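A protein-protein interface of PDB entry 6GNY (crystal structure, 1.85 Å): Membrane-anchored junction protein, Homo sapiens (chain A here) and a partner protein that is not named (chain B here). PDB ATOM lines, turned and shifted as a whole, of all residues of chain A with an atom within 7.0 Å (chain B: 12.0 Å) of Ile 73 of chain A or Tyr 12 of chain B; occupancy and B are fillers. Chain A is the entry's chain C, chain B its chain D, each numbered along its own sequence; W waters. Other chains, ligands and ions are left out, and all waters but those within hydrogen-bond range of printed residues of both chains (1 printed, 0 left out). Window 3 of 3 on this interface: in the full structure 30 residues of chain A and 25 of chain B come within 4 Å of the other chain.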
ATOM      1  N   GLN A  65      30.697  11.799 -14.561  1.00  0.00           N
ATOM      2  CA  GLN A  65      30.397  10.429 -14.176  1.00  0.00           C
ATOM      3  C   GLN A  65      29.438  10.494 -13.000  1.00  0.00           C
ATOM      4  O   GLN A  65      29.465  11.469 -12.239  1.00  0.00           O
ATOM      5  CB  GLN A  65      31.664   9.648 -13.790  1.00  0.00           C
ATOM      6  CG  GLN A  65      32.724   9.572 -14.890  1.00  0.00           C
ATOM      7  CD  GLN A  65      32.266   8.775 -16.100  1.00  0.00           C
ATOM      8  OE1 GLN A  65      31.381   7.925 -15.998  1.00  0.00           O
ATOM      9  NE2 GLN A  65      32.866   9.050 -17.255  1.00  0.00           N
ATOM     10  N   PRO A  66      28.574   9.499 -12.829  1.00  0.00           N
ATOM     11  CA  PRO A  66      27.688   9.497 -11.663  1.00  0.00           C
ATOM     12  C   PRO A  66      28.466   9.204 -10.390  1.00  0.00           C
ATOM     13  O   PRO A  66      29.550   8.620 -10.408  1.00  0.00           O
ATOM     14  CB  PRO A  66      26.682   8.385 -11.977  1.00  0.00           C
ATOM     15  CG  PRO A  66      27.426   7.459 -12.862  1.00  0.00           C
ATOM     16  CD  PRO A  66      28.415   8.281 -13.644  1.00  0.00           C
ATOM     17  N   PHE A  67      27.909   9.653  -9.268  1.00  0.00           N
ATOM     18  CA  PHE A  67      28.554   9.443  -7.983  1.00  0.00           C
ATOM     19  C   PHE A  67      27.498   9.432  -6.889  1.00  0.00           C
ATOM     20  O   PHE A  67      26.378   9.916  -7.070  1.00  0.00           O
ATOM     21  CB  PHE A  67      29.630  10.504  -7.713  1.00  0.00           C
ATOM     22  CG  PHE A  67      29.146  11.921  -7.862  1.00  0.00           C
ATOM     23  CD1 PHE A  67      29.110  12.531  -9.107  1.00  0.00           C
ATOM     24  CD2 PHE A  67      28.744  12.649  -6.755  1.00  0.00           C
ATOM     25  CE1 PHE A  67      28.676  13.836  -9.244  1.00  0.00           C
ATOM     26  CE2 PHE A  67      28.309  13.952  -6.887  1.00  0.00           C
ATOM     27  CZ  PHE A  67      28.276  14.546  -8.131  1.00  0.00           C
ATOM     28  N   ALA A  68      27.871   8.859  -5.750  1.00  0.00           N
ATOM     29  CA  ALA A  68      26.969   8.681  -4.623  1.00  0.00           C
ATOM     30  C   ALA A  68      27.391   9.569  -3.461  1.00  0.00           C
ATOM     31  O   ALA A  68      28.564   9.578  -3.073  1.00  0.00           O
ATOM     32  CB  ALA A  68      26.944   7.220  -4.174  1.00  0.00           C
ATOM     33  N   THR A  69      26.436  10.315  -2.920  1.00  0.00           N
ATOM     34  CA  THR A  69      26.612  10.993  -1.648  1.00  0.00           C
ATOM     35  C   THR A  69      25.976  10.135  -0.556  1.00  0.00           C
ATOM     36  O   THR A  69      25.491   9.028  -0.805  1.00  0.00           O
ATOM     37  CB  THR A  69      26.004  12.398  -1.693  1.00  0.00           C
ATOM     38  OG1 THR A  69      24.575  12.309  -1.754  1.00  0.00           O
ATOM     39  CG2 THR A  69      26.507  13.155  -2.912  1.00  0.00           C
ATOM     40  N   GLU A  70      25.969  10.653   0.671  1.00  0.00           N
ATOM     41  CA  GLU A  70      25.385   9.895   1.771  1.00  0.00           C
ATOM     42  C   GLU A  70      23.905   9.629   1.529  1.00  0.00           C
ATOM     43  O   GLU A  70      23.392   8.569   1.906  1.00  0.00           O
ATOM     44  CB  GLU A  70      25.574  10.637   3.095  1.00  0.00           C
ATOM     45  CG  GLU A  70      25.031   9.872   4.300  1.00  0.00           C
ATOM     46  CD  GLU A  70      25.265  10.591   5.614  1.00  0.00           C
ATOM     47  OE1 GLU A  70      25.709  11.759   5.588  1.00  0.00           O
ATOM     48  OE2 GLU A  70      25.006   9.986   6.677  1.00  0.00           O
ATOM     49  N   HIS A  71      23.203  10.574   0.902  1.00  0.00           N
ATOM     50  CA  HIS A  71      21.763  10.463   0.724  1.00  0.00           C
ATOM     51  C   HIS A  71      21.324  10.316  -0.725  1.00  0.00           C
ATOM     52  O   HIS A  71      20.167   9.950  -0.958  1.00  0.00           O
ATOM     53  CB  HIS A  71      21.064  11.691   1.329  1.00  0.00           C
ATOM     54  CG  HIS A  71      21.325  11.872   2.791  1.00  0.00           C
ATOM     55  ND1 HIS A  71      22.442  12.521   3.271  1.00  0.00           N
ATOM     56  CD2 HIS A  71      20.615  11.493   3.880  1.00  0.00           C
ATOM     57  CE1 HIS A  71      22.412  12.529   4.591  1.00  0.00           C
ATOM     58  NE2 HIS A  71      21.312  11.913   4.986  1.00  0.00           N
ATOM     59  N   PHE A  72      22.198  10.572  -1.699  1.00  0.00           N
ATOM     60  CA  PHE A  72      21.775  10.634  -3.093  1.00  0.00           C
ATOM     61  C   PHE A  72      22.738   9.876  -3.992  1.00  0.00           C
ATOM     62  O   PHE A  72      23.901   9.652  -3.653  1.00  0.00           O
ATOM     63  CB  PHE A  72      21.702  12.075  -3.608  1.00  0.00           C
ATOM     64  CG  PHE A  72      20.991  13.009  -2.695  1.00  0.00           C
ATOM     65  CD1 PHE A  72      19.655  12.823  -2.395  1.00  0.00           C
ATOM     66  CD2 PHE A  72      21.658  14.086  -2.139  1.00  0.00           C
ATOM     67  CE1 PHE A  72      18.999  13.692  -1.552  1.00  0.00           C
ATOM     68  CE2 PHE A  72      21.007  14.955  -1.297  1.00  0.00           C
ATOM     69  CZ  PHE A  72      19.673  14.759  -1.004  1.00  0.00           C
ATOM     70  N   ILE A  73      22.222   9.492  -5.155  1.00  0.00           N
ATOM     71  CA  ILE A  73      23.029   9.219  -6.336  1.00  0.00           C
ATOM     72  C   ILE A  73      22.820  10.384  -7.293  1.00  0.00           C
ATOM     73  O   ILE A  73      21.675  10.761  -7.572  1.00  0.00           O
ATOM     74  CB  ILE A  73      22.644   7.883  -6.996  1.00  0.00           C
ATOM     75  CG1 ILE A  73      22.668   6.754  -5.963  1.00  0.00           C
ATOM     76  CG2 ILE A  73      23.602   7.566  -8.134  1.00  0.00           C
ATOM     77  CD1 ILE A  73      22.163   5.428  -6.491  1.00  0.00           C
ATOM     78  N   VAL A  74      23.912  10.959  -7.791  1.00  0.00           N
ATOM     79  CA  VAL A  74      23.855  12.090  -8.710  1.00  0.00           C
ATOM     80  C   VAL A  74      24.316  11.637 -10.089  1.00  0.00           C
ATOM     81  O   VAL A  74      25.417  11.091 -10.235  1.00  0.00           O
ATOM     82  CB  VAL A  74      24.710  13.267  -8.215  1.00  0.00           C
ATOM     83  CG1 VAL A  74      24.666  14.400  -9.231  1.00  0.00           C
ATOM     84  CG2 VAL A  74      24.225  13.739  -6.847  1.00  0.00           C
ATOM     85  N   PHE A  75      23.477  11.882 -11.100  1.00  0.00           N
ATOM     86  CA  PHE A  75      23.790  11.623 -12.502  1.00  0.00           C
ATOM     87  C   PHE A  75      23.945  12.953 -13.233  1.00  0.00           C
ATOM     88  O   PHE A  75      22.950  13.527 -13.699  1.00  0.00           O
ATOM     89  CB  PHE A  75      22.687  10.786 -13.154  1.00  0.00           C
ATOM     90  CG  PHE A  75      22.499   9.424 -12.538  1.00  0.00           C
ATOM     91  CD1 PHE A  75      23.176   8.326 -13.039  1.00  0.00           C
ATOM     92  CD2 PHE A  75      21.634   9.241 -11.471  1.00  0.00           C
ATOM     93  CE1 PHE A  75      22.998   7.069 -12.487  1.00  0.00           C
ATOM     94  CE2 PHE A  75      21.453   7.990 -10.912  1.00  0.00           C
ATOM     95  CZ  PHE A  75      22.137   6.902 -11.421  1.00  0.00           C
ATOM     96  N   TYR A 106      20.755  15.168 -12.194  1.00  0.00           N
ATOM     97  CA  TYR A 106      19.599  14.343 -11.857  1.00  0.00           C
ATOM     98  C   TYR A 106      19.909  13.686 -10.519  1.00  0.00           C
ATOM     99  O   TYR A 106      20.704  12.748 -10.446  1.00  0.00           O
ATOM    100  CB  TYR A 106      19.317  13.316 -12.948  1.00  0.00           C
ATOM    101  CG  TYR A 106      18.977  13.938 -14.285  1.00  0.00           C
ATOM    102  CD1 TYR A 106      19.955  14.128 -15.248  1.00  0.00           C
ATOM    103  CD2 TYR A 106      17.679  14.332 -14.583  1.00  0.00           C
ATOM    104  CE1 TYR A 106      19.654  14.692 -16.472  1.00  0.00           C
ATOM    105  CE2 TYR A 106      17.369  14.905 -15.805  1.00  0.00           C
ATOM    106  CZ  TYR A 106      18.361  15.080 -16.746  1.00  0.00           C
ATOM    107  OH  TYR A 106      18.062  15.642 -17.967  1.00  0.00           O
ATOM    108  N   VAL A 107      19.299  14.192  -9.451  1.00  0.00           N
ATOM    109  CA  VAL A 107      19.559  13.695  -8.103  1.00  0.00           C
ATOM    110  C   VAL A 107      18.528  12.616  -7.796  1.00  0.00           C
ATOM    111  O   VAL A 107      17.320  12.877  -7.806  1.00  0.00           O
ATOM    112  CB  VAL A 107      19.505  14.832  -7.071  1.00  0.00           C
ATOM    113  CG1 VAL A 107      19.790  14.302  -5.671  1.00  0.00           C
ATOM    114  CG2 VAL A 107      20.506  15.919  -7.439  1.00  0.00           C
ATOM    115  N   GLU A 108      19.006  11.407  -7.517  1.00  0.00           N
ATOM    116  CA  GLU A 108      18.127  10.256  -7.329  1.00  0.00           C
ATOM    117  C   GLU A 108      18.354   9.577  -5.986  1.00  0.00           C
ATOM    118  O   GLU A 108      19.431   9.663  -5.394  1.00  0.00           O
ATOM    119  CB  GLU A 108      18.337   9.246  -8.461  1.00  0.00           C
ATOM    120  CG  GLU A 108      17.807   9.712  -9.810  1.00  0.00           C
ATOM    121  CD  GLU A 108      16.290   9.669  -9.895  1.00  0.00           C
ATOM    122  OE1 GLU A 108      15.660   8.925  -9.112  1.00  0.00           O
ATOM    123  OE2 GLU A 108      15.725  10.389 -10.743  1.00  0.00           O
ATOM    124  OXT GLU A 108      17.455   8.920  -5.466  1.00  0.00           O
ATOM    125  N   GLY B  11      26.400   0.776  -5.996  1.00  0.00           N
ATOM    126  CA  GLY B  11      27.341   0.376  -7.025  1.00  0.00           C
ATOM    127  C   GLY B  11      27.913   1.554  -7.791  1.00  0.00           C
ATOM    128  O   GLY B  11      28.383   1.404  -8.918  1.00  0.00           O
ATOM    129  N   TYR B  12      27.863   2.732  -7.177  1.00  0.00           N
ATOM    130  CA  TYR B  12      28.399   3.951  -7.763  1.00  0.00           C
ATOM    131  C   TYR B  12      29.585   4.444  -6.943  1.00  0.00           C
ATOM    132  O   TYR B  12      29.684   4.183  -5.739  1.00  0.00           O
ATOM    133  CB  TYR B  12      27.315   5.035  -7.843  1.00  0.00           C
ATOM    134  CG  TYR B  12      26.194   4.687  -8.803  1.00  0.00           C
ATOM    135  CD1 TYR B  12      26.295   4.981 -10.158  1.00  0.00           C
ATOM    136  CD2 TYR B  12      25.043   4.050  -8.358  1.00  0.00           C
ATOM    137  CE1 TYR B  12      25.281   4.659 -11.039  1.00  0.00           C
ATOM    138  CE2 TYR B  12      24.022   3.724  -9.234  1.00  0.00           C
ATOM    139  CZ  TYR B  12      24.147   4.032 -10.573  1.00  0.00           C
ATOM    140  OH  TYR B  12      23.135   3.712 -11.448  1.00  0.00           O
ATOM    141  N   ILE B  13      30.497   5.150  -7.611  1.00  0.00           N
ATOM    142  CA  ILE B  13      31.686   5.665  -6.942  1.00  0.00           C
ATOM    143  C   ILE B  13      31.283   6.718  -5.917  1.00  0.00           C
ATOM    144  O   ILE B  13      30.357   7.509  -6.139  1.00  0.00           O
ATOM    145  CB  ILE B  13      32.675   6.240  -7.972  1.00  0.00           C
ATOM    146  CG1 ILE B  13      33.974   6.662  -7.281  1.00  0.00           C
ATOM    147  CG2 ILE B  13      32.058   7.422  -8.710  1.00  0.00           C
ATOM    148  CD1 ILE B  13      35.054   7.130  -8.234  1.00  0.00           C
ATOM    149  N   SER B  14      31.977   6.730  -4.783  1.00  0.00           N
ATOM    150  CA  SER B  14      31.689   7.709  -3.744  1.00  0.00           C
ATOM    151  C   SER B  14      32.145   9.099  -4.168  1.00  0.00           C
ATOM    152  O   SER B  14      33.184   9.261  -4.815  1.00  0.00           O
ATOM    153  CB  SER B  14      32.373   7.317  -2.436  1.00  0.00           C
ATOM    154  OG  SER B  14      32.196   8.330  -1.459  1.00  0.00           O
ATOM    155  N   ILE B  15      31.356  10.112  -3.798  1.00  0.00           N
ATOM    156  CA  ILE B  15      31.753  11.495  -4.045  1.00  0.00           C
ATOM    157  C   ILE B  15      33.126  11.782  -3.451  1.00  0.00           C
ATOM    158  O   ILE B  15      33.884  12.604  -3.982  1.00  0.00           O
ATOM    159  CB  ILE B  15      30.689  12.466  -3.489  1.00  0.00           C
ATOM    160  CG1 ILE B  15      30.997  13.897  -3.932  1.00  0.00           C
ATOM    161  CG2 ILE B  15      30.633  12.389  -1.966  1.00  0.00           C
ATOM    162  CD1 ILE B  15      29.932  14.904  -3.552  1.00  0.00           C
ATOM    163  N   ASP B  16      33.476  11.112  -2.351  1.00  0.00           N
ATOM    164  CA  ASP B  16      34.739  11.386  -1.676  1.00  0.00           C
ATOM    165  C   ASP B  16      35.951  10.887  -2.454  1.00  0.00           C
ATOM    166  O   ASP B  16      37.079  11.239  -2.092  1.00  0.00           O
ATOM    167  CB  ASP B  16      34.733  10.754  -0.283  1.00  0.00           C
ATOM    168  CG  ASP B  16      33.672  11.351   0.621  1.00  0.00           C
ATOM    169  OD1 ASP B  16      33.475  12.585   0.578  1.00  0.00           O
ATOM    170  OD2 ASP B  16      33.036  10.587   1.377  1.00  0.00           O
ATOM    171  N   ALA B  17      35.754  10.089  -3.501  1.00  0.00           N
ATOM    172  CA  ALA B  17      36.847   9.650  -4.357  1.00  0.00           C
ATOM    173  C   ALA B  17      37.009  10.522  -5.594  1.00  0.00           C
ATOM    174  O   ALA B  17      37.863  10.228  -6.436  1.00  0.00           O
ATOM    175  CB  ALA B  17      36.635   8.194  -4.780  1.00  0.00           C
ATOM    176  N   MET B  18      36.223  11.587  -5.717  1.00  0.00           N
ATOM    177  CA  MET B  18      36.200  12.416  -6.911  1.00  0.00           C
ATOM    178  C   MET B  18      37.006  13.692  -6.708  1.00  0.00           C
ATOM    179  O   MET B  18      37.099  14.222  -5.599  1.00  0.00           O
ATOM    180  CB  MET B  18      34.760  12.787  -7.280  1.00  0.00           C
ATOM    181  CG  MET B  18      33.847  11.594  -7.508  1.00  0.00           C
ATOM    182  SD  MET B  18      34.157  10.807  -9.094  1.00  0.00           S
ATOM    183  CE  MET B  18      33.245  11.889 -10.189  1.00  0.00           C
HETATM  184  O   HOH W   1      29.495   8.555  -0.725  1.00  0.00           O
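O of Ile 13 of chain B sits at hydrogen-bond distance from N of Ala 68 of chain A. O of Ala 68 of chain A sits at hydrogen-bond distance from N of Ile 15 of chain B (2.9 Å).
O of Phe 67 of chain A sits at hydrogen-bond distance from N of Val 74 of chain A, 2.8 Å away. OG1 of Thr 69 of chain A sits close to N of His 71 of chain A (3.5 Å). N of Phe 72 of chain A sits at hydrogen-bond distance from OG1 of Thr 69 of chain A. The backbone carbonyl oxygen of Ile 73 of chain A is in hydrogen-bond range of the backbone NH of Glu 108 of chain A (2.7 Å). The backbone NH of Phe 75 of chain A lies within hydrogen-bond range of the backbone carbonyl oxygen of Tyr 106 of chain A, 3.0 Å away. OG of Ser 14 of chain B lies close to N of Asp 16 of chain B, at 3.2 Å.
Among the printed residues, merely in contact across the chains: Phe 67 of chain A with Ile 13 of chain B, Pro 66 of chain A with Ile 13 of chain B, Phe 75 of chain A with Tyr 12 of chain B, Ile 73 of chain A with Tyr 12 of chain B, Ala 68 of chain A with Ser 14 of chain B, Phe 67 of chain A with Ile 15 of chain B, Pro 66 of chain A with Tyr 12 of chain B and Thr 69 of chain A with Ile 15 of chain B.
Printed residues of chain B within 4 Å of Pro 66 of chain A: Tyr 12 and Ile 13. Printed residues of chain B within 4 Å of Ala 68 of chain A: Ile 13, Ser 14 and Ile 15. No residue of chain B comes within 4 Å of Phe 72 of chain A. Ile 73 of chain A touches just one residue of chain B: Tyr 12 (3.7 Å). No residue of chain B comes within 4 Å of Val 74 of chain A. Phe 75 of chain A touches just one residue of chain B: Tyr 12 (3.3 Å). No residue of chain B comes within 4 Å of Val 107 of chain A. No residue of chain B comes within 4 Å of Glu 108 of chain A. Tyr 12 of chain B touches three residues of chain A. Printed residues of chain A within 4 Å of Ile 13 of chain B: Pro 66 (3.3 Å), Phe 67 (3.2 Å) and Ala 68 (2.9 Å). Of the printed residues of chain A, Ser 14 of chain B touches Ala 68 (3.7 Å). Printed residues of chain A within 4 Å of Ile 15 of chain B: Phe 67 (3.8 Å), Ala 68 (2.9 Å) and Thr 69 (3.9 Å). The nearest residue of chain A that does not touch Tyr 12 of chain B is Ala 68 of chain A (4.3 Å). The nearest printed residue of chain A that does not touch Ile 13 of chain B is Gln 65 of chain A (5.6 Å).
Along chain B the printed residues that touch a printed residue of chain A span positions 12 to 15. Among the printed residues, no Asp or Glu carboxylate lies within 4 Å of a Lys or Arg side-chain nitrogen of the other chain.
Water W1 lies within hydrogen-bond range of O of Ala 68 of chain A (2.7 Å) and OG of Ser 14 of chain B (2.8 Å).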
